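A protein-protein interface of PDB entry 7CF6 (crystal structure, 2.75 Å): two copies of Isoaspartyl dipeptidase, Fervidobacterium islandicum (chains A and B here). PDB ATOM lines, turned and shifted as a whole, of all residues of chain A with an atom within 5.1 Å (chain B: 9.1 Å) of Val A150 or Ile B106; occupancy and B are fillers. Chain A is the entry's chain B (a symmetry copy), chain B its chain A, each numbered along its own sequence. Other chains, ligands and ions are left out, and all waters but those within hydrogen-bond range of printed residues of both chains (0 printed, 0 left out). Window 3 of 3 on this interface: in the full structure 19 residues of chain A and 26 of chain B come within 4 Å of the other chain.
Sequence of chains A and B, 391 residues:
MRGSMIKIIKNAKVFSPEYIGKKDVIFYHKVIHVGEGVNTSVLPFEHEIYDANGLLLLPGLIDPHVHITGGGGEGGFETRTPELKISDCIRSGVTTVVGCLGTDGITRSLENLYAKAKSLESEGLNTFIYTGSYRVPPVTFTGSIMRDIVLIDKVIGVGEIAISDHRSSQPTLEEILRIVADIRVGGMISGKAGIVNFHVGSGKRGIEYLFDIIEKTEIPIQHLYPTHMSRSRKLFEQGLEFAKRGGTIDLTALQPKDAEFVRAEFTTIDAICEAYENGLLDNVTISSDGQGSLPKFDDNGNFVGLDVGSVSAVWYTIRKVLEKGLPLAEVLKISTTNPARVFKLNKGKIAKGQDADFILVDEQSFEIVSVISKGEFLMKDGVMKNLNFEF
The backbone NH of Thr B107 lies within hydrogen-bond range of the side-chain carboxylate of Asp B104, at 2.9 Å.
O of Ile A149 sits at hydrogen-bond distance from OG of Ser A190, 3.4 Å away.
The side-chain carboxylate (OD1) of Asp B104 lies within hydrogen-bond range of the backbone NH (N) of Ile B106 (2.9 Å).
No position is printed for both chains.
Printed residues of chain B within 4 Å of Met A146: Ile B106 (3.9 Å) and Arg B135 (3.8 Å).
Of chain B, only Ile B106 comes within 4 Å of Val A150.
Of the printed residues of chain B, Ile A189 touches Gly B73 (3.5 Å), Phe B77 (3.6 Å) and Asp B104 (3.9 Å).
Printed residues of chain B within 4 Å of Ser A190: Phe B77.
Of the printed residues of chain A, Phe B77 touches Ile A189 and Ser A190.
Thr B103 touches none of the printed residues of chain A.
Ile B106 touches two residues of chain A.
Ser B109 touches none of the printed residues of chain A.
Of the printed residues of chain A, Arg B135 touches Met A146 (3.8 Å).
The nearest residue of chain B that does not touch Val A150 is Phe B77 (4.1 Å).
The nearest residue of chain A that does not touch Ile B106 is Arg A147 (4.05 Å).
The nearest printed residue of chain B that does not touch Met A146 is Thr B103 (5.9 Å).
Among the printed residues, merely in contact across the chains: Ile A189 with Gly B73 (3.5 Å), Ile A189 with Phe B77 (3.6 Å), Met A146 with Arg B135 (3.8 Å), Val A150 with Ile B106 (3.8 Å), Ile A189 with Asp B104 (3.9 Å), Met A146 with Ile B106 (3.9 Å) and Ser A190 with Phe B77 (3.9 Å).
Hydrophobic or aromatic side chains of chain B that line the printed part of chain A: Phe B77 and Ile B106.
Along chain B the printed residues that touch a printed residue of chain A span positions 73 to 135.
Among the printed residues, no Asp or Glu carboxylate lies within 4 Å of a Lys or Arg side-chain nitrogen of the other chain.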
ATOM      1  N   MET A 146      15.832  18.381  31.888  1.00  0.00           N
ATOM      2  CA  MET A 146      15.471  19.073  30.616  1.00  0.00           C
ATOM      3  C   MET A 146      14.988  20.511  30.905  1.00  0.00           C
ATOM      4  O   MET A 146      15.361  21.416  30.126  1.00  0.00           O
ATOM      5  CB  MET A 146      14.407  18.321  29.796  1.00  0.00           C
ATOM      6  CG  MET A 146      14.384  18.760  28.336  1.00  0.00           C
ATOM      7  SD  MET A 146      12.861  18.417  27.439  1.00  0.00           S
ATOM      8  CE  MET A 146      13.075  16.689  27.022  1.00  0.00           C
ATOM      9  N   ARG A 147      14.178  20.740  31.950  1.00  0.00           N
ATOM     10  CA  ARG A 147      13.797  22.124  32.346  1.00  0.00           C
ATOM     11  C   ARG A 147      15.054  22.889  32.759  1.00  0.00           C
ATOM     12  O   ARG A 147      15.203  24.006  32.268  1.00  0.00           O
ATOM     13  CB  ARG A 147      12.773  22.162  33.478  1.00  0.00           C
ATOM     14  CG  ARG A 147      11.344  21.871  33.039  1.00  0.00           C
ATOM     15  CD  ARG A 147      10.355  21.914  34.202  1.00  0.00           C
ATOM     16  NE  ARG A 147       9.880  23.263  34.472  1.00  0.00           N
ATOM     17  CZ  ARG A 147       8.940  23.887  33.765  1.00  0.00           C
ATOM     18  NH1 ARG A 147       8.366  23.277  32.725  1.00  0.00           N
ATOM     19  NH2 ARG A 147       8.593  25.126  34.118  1.00  0.00           N
ATOM     20  N   ASP A 148      15.924  22.294  33.587  1.00  0.00           N
ATOM     21  CA  ASP A 148      17.127  22.969  34.146  1.00  0.00           C
ATOM     22  C   ASP A 148      17.966  23.574  33.002  1.00  0.00           C
ATOM     23  O   ASP A 148      18.396  24.740  33.135  1.00  0.00           O
ATOM     24  CB  ASP A 148      17.966  22.022  35.014  1.00  0.00           C
ATOM     25  CG  ASP A 148      17.454  21.744  36.424  1.00  0.00           C
ATOM     26  OD1 ASP A 148      16.343  22.198  36.755  1.00  0.00           O
ATOM     27  OD2 ASP A 148      18.175  21.049  37.184  1.00  0.00           O
ATOM     28  N   ILE A 149      18.182  22.839  31.908  1.00  0.00           N
ATOM     29  CA  ILE A 149      19.107  23.242  30.803  1.00  0.00           C
ATOM     30  C   ILE A 149      18.443  24.282  29.876  1.00  0.00           C
ATOM     31  O   ILE A 149      19.181  25.052  29.168  1.00  0.00           O
ATOM     32  CB  ILE A 149      19.582  22.002  30.015  1.00  0.00           C
ATOM     33  CG1 ILE A 149      20.891  22.282  29.278  1.00  0.00           C
ATOM     34  CG2 ILE A 149      18.498  21.521  29.062  1.00  0.00           C
ATOM     35  CD1 ILE A 149      21.613  21.053  28.859  1.00  0.00           C
ATOM     36  N   VAL A 150      17.113  24.291  29.826  1.00  0.00           N
ATOM     37  CA  VAL A 150      16.315  25.241  28.994  1.00  0.00           C
ATOM     38  C   VAL A 150      16.237  26.621  29.681  1.00  0.00           C
ATOM     39  O   VAL A 150      16.224  27.636  28.939  1.00  0.00           O
ATOM     40  CB  VAL A 150      14.926  24.644  28.672  1.00  0.00           C
ATOM     41  CG1 VAL A 150      13.920  25.663  28.140  1.00  0.00           C
ATOM     42  CG2 VAL A 150      15.063  23.482  27.693  1.00  0.00           C
ATOM     43  N   LEU A 151      16.180  26.692  31.019  1.00  0.00           N
ATOM     44  CA  LEU A 151      15.877  27.968  31.739  1.00  0.00           C
ATOM     45  C   LEU A 151      17.156  28.564  32.345  1.00  0.00           C
ATOM     46  O   LEU A 151      17.306  29.810  32.298  1.00  0.00           O
ATOM     47  CB  LEU A 151      14.795  27.746  32.807  1.00  0.00           C
ATOM     48  CG  LEU A 151      13.426  27.222  32.328  1.00  0.00           C
ATOM     49  CD1 LEU A 151      12.409  27.254  33.451  1.00  0.00           C
ATOM     50  CD2 LEU A 151      12.873  27.981  31.134  1.00  0.00           C
ATOM     51  N   ILE A 152      18.087  27.728  32.802  1.00  0.00           N
ATOM     52  CA  ILE A 152      19.287  28.205  33.552  1.00  0.00           C
ATOM     53  C   ILE A 152      20.484  28.337  32.616  1.00  0.00           C
ATOM     54  O   ILE A 152      20.982  27.328  32.122  1.00  0.00           O
ATOM     55  CB  ILE A 152      19.583  27.296  34.756  1.00  0.00           C
ATOM     56  CG1 ILE A 152      18.381  27.277  35.702  1.00  0.00           C
ATOM     57  CG2 ILE A 152      20.864  27.755  35.444  1.00  0.00           C
ATOM     58  CD1 ILE A 152      18.666  26.721  37.064  1.00  0.00           C
ATOM     59  N   GLY A 186      16.742  18.660  25.585  1.00  0.00           N
ATOM     60  CA  GLY A 186      16.928  19.886  26.372  1.00  0.00           C
ATOM     61  C   GLY A 186      18.034  20.752  25.798  1.00  0.00           C
ATOM     62  O   GLY A 186      17.813  21.951  25.625  1.00  0.00           O
ATOM     63  N   ILE A 189      16.825  22.210  22.120  1.00  0.00           N
ATOM     64  CA  ILE A 189      15.852  23.326  22.362  1.00  0.00           C
ATOM     65  C   ILE A 189      16.576  24.643  22.742  1.00  0.00           C
ATOM     66  O   ILE A 189      16.195  25.728  22.184  1.00  0.00           O
ATOM     67  CB  ILE A 189      14.808  22.926  23.424  1.00  0.00           C
ATOM     68  CG1 ILE A 189      13.788  21.937  22.857  1.00  0.00           C
ATOM     69  CG2 ILE A 189      14.124  24.154  24.007  1.00  0.00           C
ATOM     70  CD1 ILE A 189      12.821  21.375  23.902  1.00  0.00           C
ATOM     71  N   SER A 190      17.560  24.589  23.650  1.00  0.00           N
ATOM     72  CA  SER A 190      18.187  25.797  24.242  1.00  0.00           C
ATOM     73  C   SER A 190      19.447  26.242  23.476  1.00  0.00           C
ATOM     74  O   SER A 190      20.020  27.289  23.844  1.00  0.00           O
ATOM     75  CB  SER A 190      18.483  25.564  25.683  1.00  0.00           C
ATOM     76  OG  SER A 190      19.724  24.916  25.820  1.00  0.00           O
ATOM     77  N   GLY B  72       8.598  23.066  15.892  1.00  0.00           N
ATOM     78  CA  GLY B  72      10.048  23.141  15.658  1.00  0.00           C
ATOM     79  C   GLY B  72      10.735  23.713  16.864  1.00  0.00           C
ATOM     80  O   GLY B  72      10.056  23.836  17.932  1.00  0.00           O
ATOM     81  N   GLY B  73      11.998  24.103  16.682  1.00  0.00           N
ATOM     82  CA  GLY B  73      12.871  24.610  17.757  1.00  0.00           C
ATOM     83  C   GLY B  73      14.028  23.664  18.061  1.00  0.00           C
ATOM     84  O   GLY B  73      14.687  23.882  19.096  1.00  0.00           O
ATOM     85  N   PHE B  77      16.163  28.569  19.898  1.00  0.00           N
ATOM     86  CA  PHE B  77      14.958  29.424  20.016  1.00  0.00           C
ATOM     87  C   PHE B  77      14.645  30.108  18.686  1.00  0.00           C
ATOM     88  O   PHE B  77      13.505  30.479  18.495  1.00  0.00           O
ATOM     89  CB  PHE B  77      15.155  30.442  21.135  1.00  0.00           C
ATOM     90  CG  PHE B  77      15.236  29.814  22.501  1.00  0.00           C
ATOM     91  CD1 PHE B  77      14.150  29.131  23.029  1.00  0.00           C
ATOM     92  CD2 PHE B  77      16.392  29.906  23.260  1.00  0.00           C
ATOM     93  CE1 PHE B  77      14.224  28.544  24.282  1.00  0.00           C
ATOM     94  CE2 PHE B  77      16.472  29.314  24.509  1.00  0.00           C
ATOM     95  CZ  PHE B  77      15.385  28.641  25.019  1.00  0.00           C
ATOM     96  N   ARG B  80      11.962  28.078  16.197  1.00  0.00           N
ATOM     97  CA  ARG B  80      10.516  27.994  16.540  1.00  0.00           C
ATOM     98  C   ARG B  80       9.741  28.593  15.364  1.00  0.00           C
ATOM     99  O   ARG B  80      10.062  29.768  14.986  1.00  0.00           O
ATOM    100  CB  ARG B  80      10.185  28.692  17.866  1.00  0.00           C
ATOM    101  CG  ARG B  80      11.050  28.303  19.066  1.00  0.00           C
ATOM    102  CD  ARG B  80      10.426  28.365  20.474  1.00  0.00           C
ATOM    103  NE  ARG B  80       9.527  29.496  20.738  1.00  0.00           N
ATOM    104  CZ  ARG B  80       8.407  29.469  21.499  1.00  0.00           C
ATOM    105  NH1 ARG B  80       8.005  28.375  22.130  1.00  0.00           N
ATOM    106  NH2 ARG B  80       7.669  30.557  21.635  1.00  0.00           N
ATOM    107  N   LEU B 101       1.248  18.658  19.489  1.00  0.00           N
ATOM    108  CA  LEU B 101       2.613  19.126  19.867  1.00  0.00           C
ATOM    109  C   LEU B 101       3.693  18.168  19.324  1.00  0.00           C
ATOM    110  O   LEU B 101       3.388  17.067  18.861  1.00  0.00           O
ATOM    111  CB  LEU B 101       2.709  19.270  21.391  1.00  0.00           C
ATOM    112  CG  LEU B 101       1.789  20.337  21.996  1.00  0.00           C
ATOM    113  CD1 LEU B 101       2.208  20.697  23.409  1.00  0.00           C
ATOM    114  CD2 LEU B 101       1.735  21.579  21.121  1.00  0.00           C
ATOM    115  N   GLY B 102       4.943  18.611  19.336  1.00  0.00           N
ATOM    116  CA  GLY B 102       6.071  17.853  18.778  1.00  0.00           C
ATOM    117  C   GLY B 102       7.270  17.833  19.717  1.00  0.00           C
ATOM    118  O   GLY B 102       7.114  17.508  20.909  1.00  0.00           O
ATOM    119  N   THR B 103       8.452  18.145  19.184  1.00  0.00           N
ATOM    120  CA  THR B 103       9.748  18.024  19.896  1.00  0.00           C
ATOM    121  C   THR B 103       9.712  18.875  21.174  1.00  0.00           C
ATOM    122  O   THR B 103      10.005  18.289  22.258  1.00  0.00           O
ATOM    123  CB  THR B 103      10.878  18.414  18.947  1.00  0.00           C
ATOM    124  OG1 THR B 103      10.650  17.626  17.772  1.00  0.00           O
ATOM    125  CG2 THR B 103      12.240  18.202  19.562  1.00  0.00           C
ATOM    126  N   ASP B 104       9.336  20.167  21.038  1.00  0.00           N
ATOM    127  CA  ASP B 104       9.168  21.143  22.154  1.00  0.00           C
ATOM    128  C   ASP B 104       7.818  20.928  22.865  1.00  0.00           C
ATOM    129  O   ASP B 104       6.754  21.149  22.251  1.00  0.00           O
ATOM    130  CB  ASP B 104       9.283  22.593  21.679  1.00  0.00           C
ATOM    131  CG  ASP B 104       9.598  23.585  22.793  1.00  0.00           C
ATOM    132  OD1 ASP B 104       9.420  23.230  23.999  1.00  0.00           O
ATOM    133  OD2 ASP B 104      10.041  24.711  22.453  1.00  0.00           O
ATOM    134  N   GLY B 105       7.895  20.479  24.121  1.00  0.00           N
ATOM    135  CA  GLY B 105       6.788  20.353  25.079  1.00  0.00           C
ATOM    136  C   GLY B 105       7.123  21.123  26.331  1.00  0.00           C
ATOM    137  O   GLY B 105       6.477  20.872  27.349  1.00  0.00           O
ATOM    138  N   ILE B 106       8.099  22.035  26.247  1.00  0.00           N
ATOM    139  CA  ILE B 106       8.523  22.926  27.367  1.00  0.00           C
ATOM    140  C   ILE B 106       7.979  24.339  27.145  1.00  0.00           C
ATOM    141  O   ILE B 106       7.492  24.908  28.126  1.00  0.00           O
ATOM    142  CB  ILE B 106      10.053  22.967  27.512  1.00  0.00           C
ATOM    143  CG1 ILE B 106      10.633  21.600  27.880  1.00  0.00           C
ATOM    144  CG2 ILE B 106      10.456  24.038  28.513  1.00  0.00           C
ATOM    145  CD1 ILE B 106      10.204  21.077  29.235  1.00  0.00           C
ATOM    146  N   THR B 107       8.118  24.897  25.935  1.00  0.00           N
ATOM    147  CA  THR B 107       7.710  26.290  25.581  1.00  0.00           C
ATOM    148  C   THR B 107       6.426  26.315  24.733  1.00  0.00           C
ATOM    149  O   THR B 107       5.915  27.413  24.480  1.00  0.00           O
ATOM    150  CB  THR B 107       8.841  27.042  24.857  1.00  0.00           C
ATOM    151  OG1 THR B 107       9.130  26.559  23.540  1.00  0.00           O
ATOM    152  CG2 THR B 107      10.132  27.001  25.639  1.00  0.00           C
ATOM    153  N   ARG B 108       5.919  25.164  24.285  1.00  0.00           N
ATOM    154  CA  ARG B 108       4.573  25.024  23.652  1.00  0.00           C
ATOM    155  C   ARG B 108       3.628  24.353  24.652  1.00  0.00           C
ATOM    156  O   ARG B 108       3.773  23.158  24.855  1.00  0.00           O
ATOM    157  CB  ARG B 108       4.650  24.194  22.367  1.00  0.00           C
ATOM    158  CG  ARG B 108       5.760  24.631  21.425  1.00  0.00           C
ATOM    159  CD  ARG B 108       5.377  25.873  20.657  1.00  0.00           C
ATOM    160  NE  ARG B 108       6.268  26.152  19.545  1.00  0.00           N
ATOM    161  CZ  ARG B 108       6.160  27.199  18.744  1.00  0.00           C
ATOM    162  NH1 ARG B 108       5.201  28.091  18.923  1.00  0.00           N
ATOM    163  NH2 ARG B 108       7.019  27.345  17.755  1.00  0.00           N
ATOM    164  N   SER B 109       2.712  25.108  25.260  1.00  0.00           N
ATOM    165  CA  SER B 109       1.694  24.601  26.224  1.00  0.00           C
ATOM    166  C   SER B 109       0.523  23.904  25.491  1.00  0.00           C
ATOM    167  O   SER B 109       0.175  24.275  24.343  1.00  0.00           O
ATOM    168  CB  SER B 109       1.222  25.705  27.181  1.00  0.00           C
ATOM    169  OG  SER B 109       0.274  26.576  26.582  1.00  0.00           O
ATOM    170  N   LEU B 110      -0.064  22.915  26.155  1.00  0.00           N
ATOM    171  CA  LEU B 110      -1.345  22.268  25.763  1.00  0.00           C
ATOM    172  C   LEU B 110      -2.510  23.267  25.842  1.00  0.00           C
ATOM    173  O   LEU B 110      -3.353  23.244  24.915  1.00  0.00           O
ATOM    174  CB  LEU B 110      -1.604  21.058  26.669  1.00  0.00           C
ATOM    175  CG  LEU B 110      -0.799  19.786  26.353  1.00  0.00           C
ATOM    176  CD1 LEU B 110      -1.076  18.723  27.414  1.00  0.00           C
ATOM    177  CD2 LEU B 110      -1.085  19.250  24.947  1.00  0.00           C
ATOM    178  N   GLU B 111      -2.552  24.130  26.857  1.00  0.00           N
ATOM    179  CA  GLU B 111      -3.624  25.165  26.988  1.00  0.00           C
ATOM    180  C   GLU B 111      -3.618  26.106  25.787  1.00  0.00           C
ATOM    181  O   GLU B 111      -4.722  26.426  25.343  1.00  0.00           O
ATOM    182  CB  GLU B 111      -3.492  26.023  28.243  1.00  0.00           C
ATOM    183  CG  GLU B 111      -3.545  25.213  29.522  1.00  0.00           C
ATOM    184  CD  GLU B 111      -2.259  24.493  29.891  1.00  0.00           C
ATOM    185  OE1 GLU B 111      -1.233  24.722  29.185  1.00  0.00           O
ATOM    186  OE2 GLU B 111      -2.302  23.680  30.863  1.00  0.00           O
ATOM    187  N   GLY B 132      -0.501  15.388  25.310  1.00  0.00           N
ATOM    188  CA  GLY B 132       0.899  14.908  25.275  1.00  0.00           C
ATOM    189  C   GLY B 132       1.786  15.565  24.206  1.00  0.00           C
ATOM    190  O   GLY B 132       1.435  16.622  23.641  1.00  0.00           O
ATOM    191  N   SER B 133       2.938  14.956  23.941  1.00  0.00           N
ATOM    192  CA  SER B 133       3.884  15.356  22.874  1.00  0.00           C
ATOM    193  C   SER B 133       4.815  14.169  22.587  1.00  0.00           C
ATOM    194  O   SER B 133       4.535  13.059  23.133  1.00  0.00           O
ATOM    195  CB  SER B 133       4.615  16.586  23.313  1.00  0.00           C
ATOM    196  OG  SER B 133       5.318  16.341  24.526  1.00  0.00           O
ATOM    197  N   ARG B 135       7.616  13.418  23.995  1.00  0.00           N
ATOM    198  CA  ARG B 135       8.321  12.829  25.165  1.00  0.00           C
ATOM    199  C   ARG B 135       7.415  11.864  25.932  1.00  0.00           C
ATOM    200  O   ARG B 135       6.211  12.138  26.029  1.00  0.00           O
ATOM    201  CB  ARG B 135       8.779  13.940  26.117  1.00  0.00           C
ATOM    202  CG  ARG B 135       9.621  13.477  27.302  1.00  0.00           C
ATOM    203  CD  ARG B 135      10.094  14.665  28.138  1.00  0.00           C
ATOM    204  NE  ARG B 135       9.760  14.493  29.543  1.00  0.00           N
ATOM    205  CZ  ARG B 135      10.514  13.889  30.454  1.00  0.00           C
ATOM    206  NH1 ARG B 135      11.699  13.394  30.144  1.00  0.00           N
ATOM    207  NH2 ARG B 135      10.066  13.770  31.692  1.00  0.00           N
ATOM    208  N   VAL B 139       3.047  15.071  28.594  1.00  0.00           N
ATOM    209  CA  VAL B 139       2.490  16.279  29.267  1.00  0.00           C
ATOM    210  C   VAL B 139       0.966  16.127  29.237  1.00  0.00           C
ATOM    211  O   VAL B 139       0.467  15.477  28.284  1.00  0.00           O
ATOM    212  CB  VAL B 139       2.972  17.588  28.612  1.00  0.00           C
ATOM    213  CG1 VAL B 139       4.451  17.823  28.851  1.00  0.00           C
ATOM    214  CG2 VAL B 139       2.675  17.625  27.122  1.00  0.00           C
